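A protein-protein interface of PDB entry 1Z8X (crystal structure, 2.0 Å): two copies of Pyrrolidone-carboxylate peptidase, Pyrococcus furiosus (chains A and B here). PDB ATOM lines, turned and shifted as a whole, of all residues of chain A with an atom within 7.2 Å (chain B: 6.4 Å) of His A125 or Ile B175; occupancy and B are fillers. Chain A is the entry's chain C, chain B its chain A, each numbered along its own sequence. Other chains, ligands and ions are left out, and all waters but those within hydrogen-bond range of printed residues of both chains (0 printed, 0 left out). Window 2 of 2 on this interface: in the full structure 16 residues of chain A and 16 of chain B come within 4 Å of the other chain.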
ATOM      1  N   ILE A  76     -18.482 -18.414  29.149  1.00  0.00           N
ATOM      2  CA  ILE A  76     -17.606 -17.306  29.487  1.00  0.00           C
ATOM      3  C   ILE A  76     -16.980 -16.817  28.181  1.00  0.00           C
ATOM      4  O   ILE A  76     -16.576 -17.625  27.342  1.00  0.00           O
ATOM      5  CB  ILE A  76     -16.471 -17.765  30.441  1.00  0.00           C
ATOM      6  CG1 ILE A  76     -17.058 -18.221  31.779  1.00  0.00           C
ATOM      7  CG2 ILE A  76     -15.463 -16.631  30.643  1.00  0.00           C
ATOM      8  CD1 ILE A  76     -17.758 -17.121  32.580  1.00  0.00           C
ATOM      9  N   LYS A 119      -4.180 -18.225  27.087  1.00  0.00           N
ATOM     10  CA  LYS A 119      -3.815 -19.016  28.259  1.00  0.00           C
ATOM     11  C   LYS A 119      -4.974 -19.071  29.254  1.00  0.00           C
ATOM     12  O   LYS A 119      -5.189 -20.084  29.921  1.00  0.00           O
ATOM     13  CB  LYS A 119      -2.571 -18.443  28.935  1.00  0.00           C
ATOM     14  CG  LYS A 119      -1.300 -18.647  28.125  1.00  0.00           C
ATOM     15  CD  LYS A 119      -0.066 -18.226  28.904  1.00  0.00           C
ATOM     16  CE  LYS A 119       1.198 -18.495  28.096  1.00  0.00           C
ATOM     17  NZ  LYS A 119       2.413 -18.053  28.828  1.00  0.00           N
ATOM     18  N   ILE A 120      -5.726 -17.980  29.353  1.00  0.00           N
ATOM     19  CA  ILE A 120      -6.868 -17.953  30.265  1.00  0.00           C
ATOM     20  C   ILE A 120      -7.927 -18.942  29.778  1.00  0.00           C
ATOM     21  O   ILE A 120      -8.458 -19.739  30.556  1.00  0.00           O
ATOM     22  CB  ILE A 120      -7.473 -16.532  30.353  1.00  0.00           C
ATOM     23  CG1 ILE A 120      -6.508 -15.614  31.113  1.00  0.00           C
ATOM     24  CG2 ILE A 120      -8.836 -16.579  31.043  1.00  0.00           C
ATOM     25  CD1 ILE A 120      -6.918 -14.144  31.124  1.00  0.00           C
ATOM     26  N   MET A 121      -8.229 -18.892  28.485  1.00  0.00           N
ATOM     27  CA  MET A 121      -9.224 -19.794  27.909  1.00  0.00           C
ATOM     28  C   MET A 121      -8.815 -21.252  28.129  1.00  0.00           C
ATOM     29  O   MET A 121      -9.642 -22.101  28.454  1.00  0.00           O
ATOM     30  CB  MET A 121      -9.382 -19.530  26.408  1.00  0.00           C
ATOM     31  CG  MET A 121     -10.396 -20.451  25.730  1.00  0.00           C
ATOM     32  SD  MET A 121     -10.678 -20.073  23.985  1.00  0.00           S
ATOM     33  CE  MET A 121      -9.321 -20.936  23.204  1.00  0.00           C
ATOM     34  N   LYS A 122      -7.530 -21.531  27.955  1.00  0.00           N
ATOM     35  CA  LYS A 122      -7.021 -22.885  28.121  1.00  0.00           C
ATOM     36  C   LYS A 122      -7.177 -23.385  29.560  1.00  0.00           C
ATOM     37  O   LYS A 122      -7.598 -24.520  29.783  1.00  0.00           O
ATOM     38  CB  LYS A 122      -5.558 -22.937  27.671  1.00  0.00           C
ATOM     39  CG  LYS A 122      -4.992 -24.342  27.510  1.00  0.00           C
ATOM     40  CD  LYS A 122      -4.313 -24.802  28.775  1.00  0.00           C
ATOM     41  CE  LYS A 122      -3.009 -24.057  29.002  1.00  0.00           C
ATOM     42  NZ  LYS A 122      -2.419 -24.398  30.335  1.00  0.00           N
ATOM     43  N   LYS A 123      -6.854 -22.536  30.532  1.00  0.00           N
ATOM     44  CA  LYS A 123      -6.978 -22.912  31.936  1.00  0.00           C
ATOM     45  C   LYS A 123      -8.452 -23.100  32.305  1.00  0.00           C
ATOM     46  O   LYS A 123      -8.793 -23.997  33.072  1.00  0.00           O
ATOM     47  CB  LYS A 123      -6.355 -21.844  32.841  1.00  0.00           C
ATOM     48  CG  LYS A 123      -6.201 -22.293  34.282  1.00  0.00           C
ATOM     49  CD  LYS A 123      -5.219 -23.456  34.378  1.00  0.00           C
ATOM     50  CE  LYS A 123      -5.261 -24.136  35.740  1.00  0.00           C
ATOM     51  NZ  LYS A 123      -4.934 -23.209  36.867  1.00  0.00           N
ATOM     52  N   LEU A 124      -9.323 -22.254  31.757  1.00  0.00           N
ATOM     53  CA  LEU A 124     -10.749 -22.368  32.038  1.00  0.00           C
ATOM     54  C   LEU A 124     -11.259 -23.726  31.549  1.00  0.00           C
ATOM     55  O   LEU A 124     -12.020 -24.400  32.244  1.00  0.00           O
ATOM     56  CB  LEU A 124     -11.521 -21.235  31.350  1.00  0.00           C
ATOM     57  CG  LEU A 124     -11.337 -19.836  31.951  1.00  0.00           C
ATOM     58  CD1 LEU A 124     -12.066 -18.795  31.087  1.00  0.00           C
ATOM     59  CD2 LEU A 124     -11.875 -19.826  33.373  1.00  0.00           C
ATOM     60  N   HIS A 125     -10.834 -24.126  30.354  1.00  0.00           N
ATOM     61  CA  HIS A 125     -11.247 -25.414  29.797  1.00  0.00           C
ATOM     62  C   HIS A 125     -10.761 -26.573  30.671  1.00  0.00           C
ATOM     63  O   HIS A 125     -11.481 -27.548  30.878  1.00  0.00           O
ATOM     64  CB  HIS A 125     -10.722 -25.565  28.366  1.00  0.00           C
ATOM     65  CG  HIS A 125     -11.387 -24.650  27.383  1.00  0.00           C
ATOM     66  ND1 HIS A 125     -11.027 -24.592  26.053  1.00  0.00           N
ATOM     67  CD2 HIS A 125     -12.396 -23.758  27.535  1.00  0.00           C
ATOM     68  CE1 HIS A 125     -11.783 -23.705  25.430  1.00  0.00           C
ATOM     69  NE2 HIS A 125     -12.624 -23.184  26.307  1.00  0.00           N
ATOM     70  N   GLU A 126      -9.545 -26.457  31.194  1.00  0.00           N
ATOM     71  CA  GLU A 126      -8.989 -27.489  32.061  1.00  0.00           C
ATOM     72  C   GLU A 126      -9.798 -27.599  33.352  1.00  0.00           C
ATOM     73  O   GLU A 126      -9.864 -28.665  33.965  1.00  0.00           O
ATOM     74  CB  GLU A 126      -7.528 -27.168  32.377  1.00  0.00           C
ATOM     75  CG  GLU A 126      -6.615 -27.275  31.165  1.00  0.00           C
ATOM     76  CD  GLU A 126      -5.178 -26.881  31.466  1.00  0.00           C
ATOM     77  OE1 GLU A 126      -4.322 -27.044  30.571  1.00  0.00           O
ATOM     78  OE2 GLU A 126      -4.905 -26.409  32.589  1.00  0.00           O
ATOM     79  N   ARG A 127     -10.410 -26.490  33.761  1.00  0.00           N
ATOM     80  CA  ARG A 127     -11.227 -26.460  34.970  1.00  0.00           C
ATOM     81  C   ARG A 127     -12.671 -26.863  34.670  1.00  0.00           C
ATOM     82  O   ARG A 127     -13.524 -26.848  35.556  1.00  0.00           O
ATOM     83  CB  ARG A 127     -11.212 -25.058  35.586  1.00  0.00           C
ATOM     84  CG  ARG A 127      -9.921 -24.685  36.304  1.00  0.00           C
ATOM     85  CD  ARG A 127      -9.784 -25.435  37.626  1.00  0.00           C
ATOM     86  NE  ARG A 127      -9.411 -24.539  38.720  1.00  0.00           N
ATOM     87  CZ  ARG A 127      -8.255 -23.884  38.793  1.00  0.00           C
ATOM     88  NH1 ARG A 127      -7.346 -24.022  37.834  1.00  0.00           N
ATOM     89  NH2 ARG A 127      -8.006 -23.087  39.825  1.00  0.00           N
ATOM     90  N   GLY A 128     -12.941 -27.215  33.418  1.00  0.00           N
ATOM     91  CA  GLY A 128     -14.283 -27.620  33.034  1.00  0.00           C
ATOM     92  C   GLY A 128     -15.248 -26.451  32.874  1.00  0.00           C
ATOM     93  O   GLY A 128     -16.462 -26.614  33.014  1.00  0.00           O
ATOM     94  N   ILE A 129     -14.708 -25.274  32.575  1.00  0.00           N
ATOM     95  CA  ILE A 129     -15.525 -24.083  32.395  1.00  0.00           C
ATOM     96  C   ILE A 129     -15.612 -23.682  30.926  1.00  0.00           C
ATOM     97  O   ILE A 129     -14.617 -23.271  30.327  1.00  0.00           O
ATOM     98  CB  ILE A 129     -14.953 -22.892  33.203  1.00  0.00           C
ATOM     99  CG1 ILE A 129     -14.911 -23.255  34.691  1.00  0.00           C
ATOM    100  CG2 ILE A 129     -15.805 -21.638  32.970  1.00  0.00           C
ATOM    101  CD1 ILE A 129     -14.280 -22.184  35.587  1.00  0.00           C
ATOM    102  N   PRO A 130     -16.802 -23.818  30.316  1.00  0.00           N
ATOM    103  CA  PRO A 130     -16.915 -23.433  28.907  1.00  0.00           C
ATOM    104  C   PRO A 130     -16.561 -21.959  28.713  1.00  0.00           C
ATOM    105  O   PRO A 130     -17.011 -21.090  29.468  1.00  0.00           O
ATOM    106  CB  PRO A 130     -18.370 -23.767  28.554  1.00  0.00           C
ATOM    107  CG  PRO A 130     -19.050 -24.051  29.868  1.00  0.00           C
ATOM    108  CD  PRO A 130     -17.982 -24.578  30.762  1.00  0.00           C
ATOM    109  N   ALA A 131     -15.729 -21.691  27.710  1.00  0.00           N
ATOM    110  CA  ALA A 131     -15.277 -20.336  27.437  1.00  0.00           C
ATOM    111  C   ALA A 131     -14.733 -20.224  26.022  1.00  0.00           C
ATOM    112  O   ALA A 131     -14.238 -21.198  25.457  1.00  0.00           O
ATOM    113  CB  ALA A 131     -14.190 -19.942  28.436  1.00  0.00           C
ATOM    114  N   TYR A 132     -14.829 -19.031  25.452  1.00  0.00           N
ATOM    115  CA  TYR A 132     -14.327 -18.798  24.109  1.00  0.00           C
ATOM    116  C   TYR A 132     -13.902 -17.345  23.989  1.00  0.00           C
ATOM    117  O   TYR A 132     -14.195 -16.525  24.865  1.00  0.00           O
ATOM    118  CB  TYR A 132     -15.400 -19.132  23.064  1.00  0.00           C
ATOM    119  CG  TYR A 132     -16.613 -18.225  23.103  1.00  0.00           C
ATOM    120  CD1 TYR A 132     -16.720 -17.131  22.239  1.00  0.00           C
ATOM    121  CD2 TYR A 132     -17.652 -18.458  24.007  1.00  0.00           C
ATOM    122  CE1 TYR A 132     -17.835 -16.294  22.273  1.00  0.00           C
ATOM    123  CE2 TYR A 132     -18.772 -17.624  24.048  1.00  0.00           C
ATOM    124  CZ  TYR A 132     -18.854 -16.549  23.179  1.00  0.00           C
ATOM    125  OH  TYR A 132     -19.967 -15.738  23.208  1.00  0.00           O
ATOM    126  N   ILE A 133     -13.191 -17.034  22.913  1.00  0.00           N
ATOM    127  CA  ILE A 133     -12.727 -15.677  22.678  1.00  0.00           C
ATOM    128  C   ILE A 133     -13.763 -14.937  21.837  1.00  0.00           C
ATOM    129  O   ILE A 133     -14.173 -15.419  20.782  1.00  0.00           O
ATOM    130  CB  ILE A 133     -11.358 -15.662  21.933  1.00  0.00           C
ATOM    131  CG1 ILE A 133     -10.201 -15.905  22.909  1.00  0.00           C
ATOM    132  CG2 ILE A 133     -11.118 -14.290  21.305  1.00  0.00           C
ATOM    133  CD1 ILE A 133     -10.441 -16.954  23.938  1.00  0.00           C
ATOM    134  N   VAL A 198      -9.893 -17.480  38.070  1.00  0.00           N
ATOM    135  CA  VAL A 198      -8.917 -18.172  37.233  1.00  0.00           C
ATOM    136  C   VAL A 198      -8.201 -17.182  36.316  1.00  0.00           C
ATOM    137  O   VAL A 198      -6.981 -17.247  36.138  1.00  0.00           O
ATOM    138  CB  VAL A 198      -9.590 -19.272  36.380  1.00  0.00           C
ATOM    139  CG1 VAL A 198      -8.640 -19.739  35.273  1.00  0.00           C
ATOM    140  CG2 VAL A 198      -9.964 -20.456  37.273  1.00  0.00           C
ATOM    141  N   ILE B 170     -24.101 -30.726  30.552  1.00  0.00           N
ATOM    142  CA  ILE B 170     -23.484 -30.147  31.742  1.00  0.00           C
ATOM    143  C   ILE B 170     -22.213 -29.500  31.159  1.00  0.00           C
ATOM    144  O   ILE B 170     -21.748 -29.904  30.094  1.00  0.00           O
ATOM    145  CB  ILE B 170     -23.157 -31.198  32.839  1.00  0.00           C
ATOM    146  CG1 ILE B 170     -22.327 -32.342  32.272  1.00  0.00           C
ATOM    147  CG2 ILE B 170     -24.464 -31.723  33.444  1.00  0.00           C
ATOM    148  CD1 ILE B 170     -21.922 -33.353  33.329  1.00  0.00           C
ATOM    149  N   PRO B 171     -21.656 -28.476  31.830  1.00  0.00           N
ATOM    150  CA  PRO B 171     -20.456 -27.760  31.368  1.00  0.00           C
ATOM    151  C   PRO B 171     -19.288 -28.550  30.768  1.00  0.00           C
ATOM    152  O   PRO B 171     -18.790 -28.196  29.701  1.00  0.00           O
ATOM    153  CB  PRO B 171     -20.038 -26.955  32.597  1.00  0.00           C
ATOM    154  CG  PRO B 171     -21.361 -26.655  33.255  1.00  0.00           C
ATOM    155  CD  PRO B 171     -22.066 -27.995  33.161  1.00  0.00           C
ATOM    156  N   GLU B 172     -18.843 -29.606  31.441  1.00  0.00           N
ATOM    157  CA  GLU B 172     -17.719 -30.388  30.934  1.00  0.00           C
ATOM    158  C   GLU B 172     -17.958 -30.980  29.546  1.00  0.00           C
ATOM    159  O   GLU B 172     -17.006 -31.280  28.824  1.00  0.00           O
ATOM    160  CB  GLU B 172     -17.360 -31.506  31.911  1.00  0.00           C
ATOM    161  CG  GLU B 172     -18.529 -32.383  32.315  1.00  0.00           C
ATOM    162  CD  GLU B 172     -18.194 -33.293  33.477  1.00  0.00           C
ATOM    163  OE1 GLU B 172     -17.618 -34.378  33.241  1.00  0.00           O
ATOM    164  OE2 GLU B 172     -18.496 -32.914  34.632  1.00  0.00           O
ATOM    165  N   GLN B 173     -19.224 -31.146  29.174  1.00  0.00           N
ATOM    166  CA  GLN B 173     -19.555 -31.699  27.865  1.00  0.00           C
ATOM    167  C   GLN B 173     -19.381 -30.672  26.745  1.00  0.00           C
ATOM    168  O   GLN B 173     -19.298 -31.035  25.575  1.00  0.00           O
ATOM    169  CB  GLN B 173     -21.001 -32.207  27.852  1.00  0.00           C
ATOM    170  CG  GLN B 173     -21.254 -33.436  28.709  1.00  0.00           C
ATOM    171  CD  GLN B 173     -22.678 -33.954  28.565  1.00  0.00           C
ATOM    172  OE1 GLN B 173     -23.626 -33.381  29.110  1.00  0.00           O
ATOM    173  NE2 GLN B 173     -22.836 -35.034  27.805  1.00  0.00           N
ATOM    174  N   ILE B 174     -19.324 -29.394  27.110  1.00  0.00           N
ATOM    175  CA  ILE B 174     -19.186 -28.317  26.136  1.00  0.00           C
ATOM    176  C   ILE B 174     -17.747 -28.077  25.670  1.00  0.00           C
ATOM    177  O   ILE B 174     -17.516 -27.647  24.539  1.00  0.00           O
ATOM    178  CB  ILE B 174     -19.723 -26.986  26.711  1.00  0.00           C
ATOM    179  CG1 ILE B 174     -21.153 -27.172  27.234  1.00  0.00           C
ATOM    180  CG2 ILE B 174     -19.676 -25.902  25.640  1.00  0.00           C
ATOM    181  CD1 ILE B 174     -22.148 -27.628  26.180  1.00  0.00           C
ATOM    182  N   ILE B 175     -16.787 -28.361  26.542  1.00  0.00           N
ATOM    183  CA  ILE B 175     -15.373 -28.132  26.245  1.00  0.00           C
ATOM    184  C   ILE B 175     -14.899 -28.477  24.833  1.00  0.00           C
ATOM    185  O   ILE B 175     -14.376 -27.613  24.133  1.00  0.00           O
ATOM    186  CB  ILE B 175     -14.467 -28.865  27.266  1.00  0.00           C
ATOM    187  CG1 ILE B 175     -14.933 -28.548  28.692  1.00  0.00           C
ATOM    188  CG2 ILE B 175     -13.013 -28.419  27.093  1.00  0.00           C
ATOM    189  CD1 ILE B 175     -15.066 -27.060  28.987  1.00  0.00           C
ATOM    190  N   ASP B 176     -15.074 -29.724  24.401  1.00  0.00           N
ATOM    191  CA  ASP B 176     -14.616 -30.103  23.064  1.00  0.00           C
ATOM    192  C   ASP B 176     -15.516 -29.627  21.926  1.00  0.00           C
ATOM    193  O   ASP B 176     -15.169 -29.779  20.753  1.00  0.00           O
ATOM    194  CB  ASP B 176     -14.417 -31.619  22.967  1.00  0.00           C
ATOM    195  CG  ASP B 176     -15.685 -32.397  23.240  1.00  0.00           C
ATOM    196  OD1 ASP B 176     -16.735 -32.060  22.653  1.00  0.00           O
ATOM    197  OD2 ASP B 176     -15.627 -33.358  24.035  1.00  0.00           O
ATOM    198  N   LYS B 177     -16.667 -29.052  22.268  1.00  0.00           N
ATOM    199  CA  LYS B 177     -17.596 -28.545  21.263  1.00  0.00           C
ATOM    200  C   LYS B 177     -17.061 -27.210  20.753  1.00  0.00           C
ATOM    201  O   LYS B 177     -17.135 -26.905  19.563  1.00  0.00           O
ATOM    202  CB  LYS B 177     -18.979 -28.307  21.875  1.00  0.00           C
ATOM    203  CG  LYS B 177     -19.570 -29.474  22.649  1.00  0.00           C
ATOM    204  CD  LYS B 177     -20.074 -30.569  21.737  1.00  0.00           C
ATOM    205  CE  LYS B 177     -20.764 -31.661  22.542  1.00  0.00           C
ATOM    206  NZ  LYS B 177     -21.196 -32.792  21.682  1.00  0.00           N
ATOM    207  N   ILE B 178     -16.529 -26.417  21.679  1.00  0.00           N
ATOM    208  CA  ILE B 178     -15.987 -25.096  21.379  1.00  0.00           C
ATOM    209  C   ILE B 178     -15.039 -25.104  20.180  1.00  0.00           C
ATOM    210  O   ILE B 178     -15.029 -24.167  19.379  1.00  0.00           O
ATOM    211  CB  ILE B 178     -15.264 -24.522  22.617  1.00  0.00           C
ATOM    212  CG1 ILE B 178     -16.242 -24.469  23.797  1.00  0.00           C
ATOM    213  CG2 ILE B 178     -14.715 -23.133  22.313  1.00  0.00           C
ATOM    214  CD1 ILE B 178     -15.622 -24.060  25.114  1.00  0.00           C
ATOM    215  N   GLY B 179     -14.246 -26.163  20.060  1.00  0.00           N
ATOM    216  CA  GLY B 179     -13.322 -26.267  18.944  1.00  0.00           C
ATOM    217  C   GLY B 179     -14.052 -26.514  17.633  1.00  0.00           C
ATOM    218  O   GLY B 179     -13.602 -26.080  16.569  1.00  0.00           O
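The backbone carbonyl oxygen of Ala A131 sits at hydrogen-bond distance from a ring nitrogen (NE2) of His A125.
The backbone NH (N) of Ile A76 sits at hydrogen-bond distance from the backbone carbonyl oxygen (O) of Pro A130 (3.1 Å).
The backbone NH (N) of Ile A129 is in hydrogen-bond range of the backbone carbonyl oxygen (O) of Leu A124 (2.8 Å).
Of chain B, only Ile B175 (3.9 Å) and Ile B178 (3.3 Å) come within 4 Å of His A125.
Of the printed residues of chain A, Pro B171 touches Gly A128 (3.6 Å) and Pro A130 (3.6 Å).
Printed residues of chain B within 4 Å of Ile A129: Ile B175.
Printed residues of chain A within 4 Å of Ile B174: Pro A130.
Ile A120 touches none of the printed residues of chain B.
Tyr A132 touches none of the printed residues of chain B.
The nearest printed residue of chain B that does not touch His A125 is Gly B179 (6.4 Å).
The nearest printed residue of chain B that does not touch Gly A128 is Glu B172 (4.1 Å).
Among the printed residues, pairs that only touch across the chains: His A125 with Ile B175 (3.9 Å), His A125 with Ile B178 (3.3 Å), Gly A128 with Pro B171 (3.6 Å), Gly A128 with Ile B175 (3.9 Å), Ile A129 with Ile B175 (3.9 Å), Pro A130 with Pro B171 (3.6 Å), Pro A130 with Ile B174 (3.8 Å), Pro A130 with Ile B175 (3.9 Å) and Ala A131 with Ile B178 (3.2 Å).
Printed residues of chain B that touch a printed residue of chain A: Pro B171, Ile B174, Ile B175 and Ile B178.
Among the printed residues, no Asp or Glu carboxylate lies within 4 Å of a Lys or Arg side-chain nitrogen of the other chain.
No position is printed for both chains.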
